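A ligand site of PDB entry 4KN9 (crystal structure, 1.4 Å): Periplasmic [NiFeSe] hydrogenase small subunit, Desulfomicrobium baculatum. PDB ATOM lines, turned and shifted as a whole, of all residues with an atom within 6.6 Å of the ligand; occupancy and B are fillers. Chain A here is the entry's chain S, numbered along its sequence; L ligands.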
ATOM      1  N   ILE A 207      16.127  11.616  17.788  1.00  0.00           N
ATOM      2  CA  ILE A 207      15.262  12.672  17.227  1.00  0.00           C
ATOM      3  C   ILE A 207      15.822  14.057  17.607  1.00  0.00           C
ATOM      4  O   ILE A 207      16.049  14.901  16.748  1.00  0.00           O
ATOM      5  CB  ILE A 207      13.787  12.527  17.733  1.00  0.00           C
ATOM      6  CG1 ILE A 207      13.160  11.207  17.237  1.00  0.00           C
ATOM      7  CG2 ILE A 207      12.947  13.791  17.383  1.00  0.00           C
ATOM      8  CD1 ILE A 207      12.295  11.281  16.035  1.00  0.00           C
ATOM      9  N   HIS A 208      16.067  14.266  18.897  1.00  0.00           N
ATOM     10  CA  HIS A 208      16.534  15.565  19.419  1.00  0.00           C
ATOM     11  C   HIS A 208      17.847  16.033  18.752  1.00  0.00           C
ATOM     12  O   HIS A 208      17.918  17.169  18.264  1.00  0.00           O
ATOM     13  CB  HIS A 208      16.612  15.444  20.933  1.00  0.00           C
ATOM     14  CG  HIS A 208      17.153  16.655  21.631  1.00  0.00           C
ATOM     15  ND1 HIS A 208      16.412  17.798  21.840  1.00  0.00           N
ATOM     16  CD2 HIS A 208      18.350  16.862  22.230  1.00  0.00           C
ATOM     17  CE1 HIS A 208      17.149  18.677  22.516  1.00  0.00           C
ATOM     18  NE2 HIS A 208      18.324  18.126  22.767  1.00  0.00           N
ATOM     19  N   GLU A 209      18.846  15.135  18.667  1.00  0.00           N
ATOM     20  CA  GLU A 209      20.129  15.478  18.044  1.00  0.00           C
ATOM     21  C   GLU A 209      19.952  15.921  16.597  1.00  0.00           C
ATOM     22  O   GLU A 209      20.747  16.717  16.073  1.00  0.00           O
ATOM     23  CB  GLU A 209      21.104  14.290  18.143  1.00  0.00           C
ATOM     24  CG  GLU A 209      21.580  13.988  19.566  1.00  0.00           C
ATOM     25  CD  GLU A 209      22.469  12.744  19.643  1.00  0.00           C
ATOM     26  OE1 GLU A 209      22.992  12.282  18.606  1.00  0.00           O
ATOM     27  OE2 GLU A 209      22.619  12.221  20.762  1.00  0.00           O
ATOM     28  N   CYS A 211      17.036  17.336  15.401  1.00  0.00           N
ATOM     29  CA  CYS A 211      15.838  18.158  15.335  1.00  0.00           C
ATOM     30  C   CYS A 211      16.126  19.558  14.807  1.00  0.00           C
ATOM     31  O   CYS A 211      17.102  20.191  15.221  1.00  0.00           O
ATOM     32  CB  CYS A 211      15.222  18.295  16.715  1.00  0.00           C
ATOM     33  SG  CYS A 211      13.666  19.169  16.698  1.00  0.00           S
ATOM     34  N   PRO A 212      15.276  20.062  13.902  1.00  0.00           N
ATOM     35  CA  PRO A 212      15.474  21.450  13.439  1.00  0.00           C
ATOM     36  C   PRO A 212      15.271  22.540  14.518  1.00  0.00           C
ATOM     37  O   PRO A 212      15.643  23.693  14.285  1.00  0.00           O
ATOM     38  CB  PRO A 212      14.432  21.622  12.342  1.00  0.00           C
ATOM     39  CG  PRO A 212      13.398  20.577  12.607  1.00  0.00           C
ATOM     40  CD  PRO A 212      14.141  19.409  13.223  1.00  0.00           C
ATOM     41  N   TYR A 213      14.697  22.190  15.661  1.00  0.00           N
ATOM     42  CA  TYR A 213      14.522  23.128  16.770  1.00  0.00           C
ATOM     43  C   TYR A 213      15.711  23.146  17.725  1.00  0.00           C
ATOM     44  O   TYR A 213      15.646  23.845  18.725  1.00  0.00           O
ATOM     45  CB  TYR A 213      13.259  22.816  17.583  1.00  0.00           C
ATOM     46  CG  TYR A 213      11.962  23.042  16.859  1.00  0.00           C
ATOM     47  CD1 TYR A 213      11.403  22.046  16.068  1.00  0.00           C
ATOM     48  CD2 TYR A 213      11.250  24.245  17.014  1.00  0.00           C
ATOM     49  CE1 TYR A 213      10.196  22.244  15.403  1.00  0.00           C
ATOM     50  CE2 TYR A 213      10.032  24.449  16.345  1.00  0.00           C
ATOM     51  CZ  TYR A 213       9.513  23.436  15.559  1.00  0.00           C
ATOM     52  OH  TYR A 213       8.309  23.611  14.898  1.00  0.00           O
ATOM     53  N   LEU A 214      16.742  22.353  17.440  1.00  0.00           N
ATOM     54  CA  LEU A 214      17.866  22.223  18.377  1.00  0.00           C
ATOM     55  C   LEU A 214      18.560  23.570  18.655  1.00  0.00           C
ATOM     56  O   LEU A 214      18.956  23.806  19.785  1.00  0.00           O
ATOM     57  CB  LEU A 214      18.866  21.157  17.909  1.00  0.00           C
ATOM     58  CG  LEU A 214      19.928  20.764  18.939  1.00  0.00           C
ATOM     59  CD1 LEU A 214      19.264  20.117  20.124  1.00  0.00           C
ATOM     60  CD2 LEU A 214      20.951  19.801  18.317  1.00  0.00           C
ATOM     61  N   ASP A 215      18.649  24.442  17.650  1.00  0.00           N
ATOM     62  CA  ASP A 215      19.233  25.790  17.853  1.00  0.00           C
ATOM     63  C   ASP A 215      18.435  26.586  18.897  1.00  0.00           C
ATOM     64  O   ASP A 215      18.990  27.272  19.756  1.00  0.00           O
ATOM     65  CB  ASP A 215      19.324  26.552  16.511  1.00  0.00           C
ATOM     66  CG  ASP A 215      17.938  26.813  15.852  1.00  0.00           C
ATOM     67  OD1 ASP A 215      16.976  26.008  16.004  1.00  0.00           O
ATOM     68  OD2 ASP A 215      17.826  27.840  15.139  1.00  0.00           O
ATOM     69  N   LYS A 216      17.109  26.465  18.828  1.00  0.00           N
ATOM     70  CA  LYS A 216      16.229  27.120  19.791  1.00  0.00           C
ATOM     71  C   LYS A 216      16.368  26.515  21.190  1.00  0.00           C
ATOM     72  O   LYS A 216      16.445  27.246  22.185  1.00  0.00           O
ATOM     73  CB  LYS A 216      14.780  27.049  19.280  1.00  0.00           C
ATOM     74  CG  LYS A 216      14.513  28.023  18.114  1.00  0.00           C
ATOM     75  CD  LYS A 216      13.353  27.568  17.259  1.00  0.00           C
ATOM     76  CE  LYS A 216      13.224  28.447  16.003  1.00  0.00           C
ATOM     77  NZ  LYS A 216      12.326  27.788  14.990  1.00  0.00           N
ATOM     78  N   TYR A 217      16.399  25.189  21.260  1.00  0.00           N
ATOM     79  CA  TYR A 217      16.665  24.503  22.529  1.00  0.00           C
ATOM     80  C   TYR A 217      17.963  25.036  23.176  1.00  0.00           C
ATOM     81  O   TYR A 217      17.984  25.334  24.374  1.00  0.00           O
ATOM     82  CB  TYR A 217      16.784  22.989  22.278  1.00  0.00           C
ATOM     83  CG  TYR A 217      17.163  22.188  23.494  1.00  0.00           C
ATOM     84  CD1 TYR A 217      18.500  21.934  23.792  1.00  0.00           C
ATOM     85  CD2 TYR A 217      16.180  21.657  24.340  1.00  0.00           C
ATOM     86  CE1 TYR A 217      18.868  21.185  24.910  1.00  0.00           C
ATOM     87  CE2 TYR A 217      16.527  20.900  25.453  1.00  0.00           C
ATOM     88  CZ  TYR A 217      17.872  20.676  25.733  1.00  0.00           C
ATOM     89  OH  TYR A 217      18.213  19.930  26.834  1.00  0.00           O
ATOM     90  N   PHE A 222      11.936  28.336  24.358  1.00  0.00           N
ATOM     91  CA  PHE A 222      10.940  27.297  24.480  1.00  0.00           C
ATOM     92  C   PHE A 222       9.538  27.847  24.232  1.00  0.00           C
ATOM     93  O   PHE A 222       9.158  28.895  24.769  1.00  0.00           O
ATOM     94  CB  PHE A 222      11.009  26.654  25.863  1.00  0.00           C
ATOM     95  CG  PHE A 222      12.320  26.008  26.155  1.00  0.00           C
ATOM     96  CD1 PHE A 222      12.702  24.845  25.491  1.00  0.00           C
ATOM     97  CD2 PHE A 222      13.210  26.583  27.077  1.00  0.00           C
ATOM     98  CE1 PHE A 222      13.919  24.242  25.755  1.00  0.00           C
ATOM     99  CE2 PHE A 222      14.417  25.985  27.351  1.00  0.00           C
ATOM    100  CZ  PHE A 222      14.792  24.820  26.680  1.00  0.00           C
ATOM    101  N   GLY A 230       9.410  28.353  19.241  1.00  0.00           N
ATOM    102  CA  GLY A 230      10.399  27.769  20.130  1.00  0.00           C
ATOM    103  C   GLY A 230      10.416  26.254  20.114  1.00  0.00           C
ATOM    104  O   GLY A 230       9.529  25.603  19.565  1.00  0.00           O
ATOM    105  N   CYS A 231      11.452  25.697  20.745  1.00  0.00           N
ATOM    106  CA  CYS A 231      11.572  24.275  21.009  1.00  0.00           C
ATOM    107  C   CYS A 231      10.352  23.791  21.824  1.00  0.00           C
ATOM    108  O   CYS A 231       9.794  24.547  22.637  1.00  0.00           O
ATOM    109  CB  CYS A 231      12.901  24.017  21.736  1.00  0.00           C
ATOM    110  SG  CYS A 231      12.995  22.455  22.637  1.00  0.00           S
ATOM    111  N   LYS A 232       9.949  22.553  21.591  1.00  0.00           N
ATOM    112  CA  LYS A 232       8.751  21.966  22.219  1.00  0.00           C
ATOM    113  C   LYS A 232       9.008  21.269  23.568  1.00  0.00           C
ATOM    114  O   LYS A 232       8.093  20.648  24.119  1.00  0.00           O
ATOM    115  CB  LYS A 232       8.067  20.965  21.260  1.00  0.00           C
ATOM    116  CG  LYS A 232       7.891  21.460  19.828  1.00  0.00           C
ATOM    117  CD  LYS A 232       7.029  22.734  19.774  1.00  0.00           C
ATOM    118  CE  LYS A 232       6.606  23.038  18.349  1.00  0.00           C
ATOM    119  NZ  LYS A 232       5.544  22.110  17.874  1.00  0.00           N
ATOM    120  N   ALA A 233      10.225  21.387  24.106  1.00  0.00           N
ATOM    121  CA  ALA A 233      10.592  20.620  25.294  1.00  0.00           C
ATOM    122  C   ALA A 233       9.636  20.832  26.470  1.00  0.00           C
ATOM    123  O   ALA A 233       9.262  19.876  27.141  1.00  0.00           O
ATOM    124  CB  ALA A 233      12.026  20.943  25.760  1.00  0.00           C
ATOM    125  N   GLU A 234       9.268  22.096  26.733  1.00  0.00           N
ATOM    126  CA  GLU A 234       8.417  22.382  27.887  1.00  0.00           C
ATOM    127  C   GLU A 234       6.986  21.928  27.698  1.00  0.00           C
ATOM    128  O   GLU A 234       6.238  21.828  28.686  1.00  0.00           O
ATOM    129  CB  GLU A 234       8.443  23.864  28.261  1.00  0.00           C
ATOM    130  CG  GLU A 234       9.783  24.375  28.751  1.00  0.00           C
ATOM    131  CD  GLU A 234       9.760  25.883  29.065  1.00  0.00           C
ATOM    132  OE1 GLU A 234      10.780  26.386  29.545  1.00  0.00           O
ATOM    133  OE2 GLU A 234       8.739  26.552  28.798  1.00  0.00           O
ATOM    134  N   CYS A 237       7.852  17.370  24.853  1.00  0.00           N
ATOM    135  CA  CYS A 237       8.562  16.654  23.779  1.00  0.00           C
ATOM    136  C   CYS A 237       9.505  15.555  24.290  1.00  0.00           C
ATOM    137  O   CYS A 237      10.377  15.810  25.158  1.00  0.00           O
ATOM    138  CB  CYS A 237       9.318  17.634  22.877  1.00  0.00           C
ATOM    139  SG  CYS A 237       9.991  16.845  21.421  1.00  0.00           S
ATOM    140  N   LYS A 238       9.337  14.323  23.771  1.00  0.00           N
ATOM    141  CA  LYS A 238      10.206  13.207  24.168  1.00  0.00           C
ATOM    142  C   LYS A 238      11.300  12.919  23.153  1.00  0.00           C
ATOM    143  O   LYS A 238      11.978  11.890  23.242  1.00  0.00           O
ATOM    144  CB  LYS A 238       9.397  11.929  24.474  1.00  0.00           C
ATOM    145  CG  LYS A 238       8.315  12.153  25.543  1.00  0.00           C
ATOM    146  CD  LYS A 238       8.891  12.777  26.847  1.00  0.00           C
ATOM    147  CE  LYS A 238       7.870  12.788  27.988  1.00  0.00           C
ATOM    148  NZ  LYS A 238       6.576  13.391  27.577  1.00  0.00           N
ATOM    149  N   GLY A 239      11.522  13.843  22.227  1.00  0.00           N
ATOM    150  CA  GLY A 239      12.604  13.707  21.259  1.00  0.00           C
ATOM    151  C   GLY A 239      13.954  13.382  21.885  1.00  0.00           C
ATOM    152  O   GLY A 239      14.698  12.585  21.309  1.00  0.00           O
ATOM    153  N   PRO A 240      14.306  13.983  23.051  1.00  0.00           N
ATOM    154  CA  PRO A 240      15.601  13.690  23.670  1.00  0.00           C
ATOM    155  C   PRO A 240      15.855  12.208  23.966  1.00  0.00           C
ATOM    156  O   PRO A 240      17.014  11.787  23.972  1.00  0.00           O
ATOM    157  CB  PRO A 240      15.554  14.511  24.948  1.00  0.00           C
ATOM    158  CG  PRO A 240      14.759  15.746  24.520  1.00  0.00           C
ATOM    159  CD  PRO A 240      13.648  15.133  23.718  1.00  0.00           C
ATOM    160  N   TRP A 257       5.211  16.503  10.637  1.00  0.00           N
ATOM    161  CA  TRP A 257       5.655  15.476  11.603  1.00  0.00           C
ATOM    162  C   TRP A 257       5.321  15.936  13.006  1.00  0.00           C
ATOM    163  O   TRP A 257       4.923  17.100  13.208  1.00  0.00           O
ATOM    164  CB  TRP A 257       7.134  15.106  11.429  1.00  0.00           C
ATOM    165  CG  TRP A 257       8.136  16.179  11.835  1.00  0.00           C
ATOM    166  CD1 TRP A 257       8.240  17.457  11.327  1.00  0.00           C
ATOM    167  CD2 TRP A 257       9.218  16.020  12.767  1.00  0.00           C
ATOM    168  NE1 TRP A 257       9.321  18.101  11.899  1.00  0.00           N
ATOM    169  CE2 TRP A 257       9.925  17.253  12.792  1.00  0.00           C
ATOM    170  CE3 TRP A 257       9.651  14.968  13.579  1.00  0.00           C
ATOM    171  CZ2 TRP A 257      11.068  17.452  13.603  1.00  0.00           C
ATOM    172  CZ3 TRP A 257      10.768  15.156  14.392  1.00  0.00           C
ATOM    173  CH2 TRP A 257      11.469  16.399  14.406  1.00  0.00           C
ATOM    174  N   VAL A 259       6.837  16.673  15.811  1.00  0.00           N
ATOM    175  CA  VAL A 259       7.530  17.735  16.531  1.00  0.00           C
ATOM    176  C   VAL A 259       7.182  19.107  15.951  1.00  0.00           C
ATOM    177  O   VAL A 259       6.941  20.042  16.707  1.00  0.00           O
ATOM    178  CB  VAL A 259       9.053  17.496  16.552  1.00  0.00           C
ATOM    179  CG1 VAL A 259       9.810  18.726  17.062  1.00  0.00           C
ATOM    180  CG2 VAL A 259       9.389  16.239  17.385  1.00  0.00           C
ATOM    181  N   ALA A 262       3.408  19.493  17.048  1.00  0.00           N
ATOM    182  CA  ALA A 262       3.061  19.370  18.471  1.00  0.00           C
ATOM    183  C   ALA A 262       4.267  18.906  19.267  1.00  0.00           C
ATOM    184  O   ALA A 262       5.161  19.685  19.479  1.00  0.00           O
ATOM    185  CB  ALA A 262       1.860  18.415  18.656  1.00  0.00           C
ATOM    186  N   VAL A 263       4.288  17.646  19.698  1.00  0.00           N
ATOM    187  CA  VAL A 263       5.428  17.070  20.416  1.00  0.00           C
ATOM    188  C   VAL A 263       5.660  15.622  19.959  1.00  0.00           C
ATOM    189  O   VAL A 263       4.721  14.958  19.461  1.00  0.00           O
ATOM    190  CB  VAL A 263       5.177  17.019  21.957  1.00  0.00           C
ATOM    191  CG1 VAL A 263       5.194  18.441  22.569  1.00  0.00           C
ATOM    192  CG2 VAL A 263       3.840  16.315  22.293  1.00  0.00           C
ATOM    193  N   CYS A 264       6.902  15.152  20.087  1.00  0.00           N
ATOM    194  CA  CYS A 264       7.192  13.725  19.986  1.00  0.00           C
ATOM    195  C   CYS A 264       6.691  13.050  21.269  1.00  0.00           C
ATOM    196  O   CYS A 264       6.940  13.561  22.381  1.00  0.00           O
ATOM    197  CB  CYS A 264       8.708  13.506  19.815  1.00  0.00           C
ATOM    198  SG  CYS A 264       9.177  11.740  19.731  1.00  0.00           S
HETATM  199 FE1  LIG L   1      13.140  20.631  21.279  1.00  0.00          FE
HETATM  200 FE2  LIG L   1      13.358  19.211  18.968  1.00  0.00          FE
HETATM  201 FE3  LIG L   1      14.543  18.395  21.166  1.00  0.00          FE
HETATM  202 FE4  LIG L   1      11.830  18.213  20.992  1.00  0.00          FE
HETATM  203  S1  LIG L   1      13.372  17.034  19.757  1.00  0.00           S
HETATM  204  S2  LIG L   1      12.999  18.885  22.795  1.00  0.00           S
HETATM  205  S3  LIG L   1      11.472  20.176  19.838  1.00  0.00           S
HETATM  206  S4  LIG L   1      15.017  20.334  20.036  1.00  0.00           S
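Tyr 213 touches the ligand. Tyr 217 touches the ligand. Ala 233 touches the ligand. Gly 239 touches the ligand. Pro 240 touches the ligand. Val 259 touches the ligand. Hydrophobic or aromatic side chains that line the ligand: His 208, Tyr 213, Tyr 217, Ala 233, Pro 240 and Val 259. Of the 25 residues printed, 12 come within 4 Å of the ligand. Along chain A the residues within 4 Å of the ligand span positions 208 to 259.
A ring nitrogen (ND1) of His 208 is bound to an iron atom (FE3) of the ligand, 2.1 Å away. FE1 of the ligand is bound by SG of Cys 231. An iron atom (FE2) of the ligand is bound by the side-chain sulfur of Cys 211, at 2.3 Å. SG of Cys 237 is bound to FE4 of the ligand (2.3 Å). The backbone NH (N) of Lys 232 lies close to a sulfur (S3) of the ligand, at 3.3 Å. N of Leu 214 lies close to S4 of the ligand, at 3.7 Å.
The backbone NH of His 208 is in hydrogen-bond range of the backbone carbonyl oxygen of Gly 239 (3.2 Å). SG of Cys 231 lies close to N of Ala 233, at 3.3 Å. The side-chain sulfur (SG) of Cys 211 sits close to the backbone NH (N) of Tyr 213 (3.4 Å). The backbone carbonyl oxygen of Lys 232 is in hydrogen-bond range of the backbone NH of Cys 237 (3.4 Å). The side-chain sulfur (SG) of Cys 237 sits close to the backbone NH (N) of Gly 239, at 3.5 Å. SG of Cys 237 sits close to N of Cys 264. The side-chain amino group of Lys 232 is in hydrogen-bond range of the backbone carbonyl oxygen of Val 259 (2.8 Å). The backbone carbonyl oxygen (O) of Ala 262 lies within hydrogen-bond range of the side-chain amino group (NZ) of Lys 232, at 2.9 Å.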
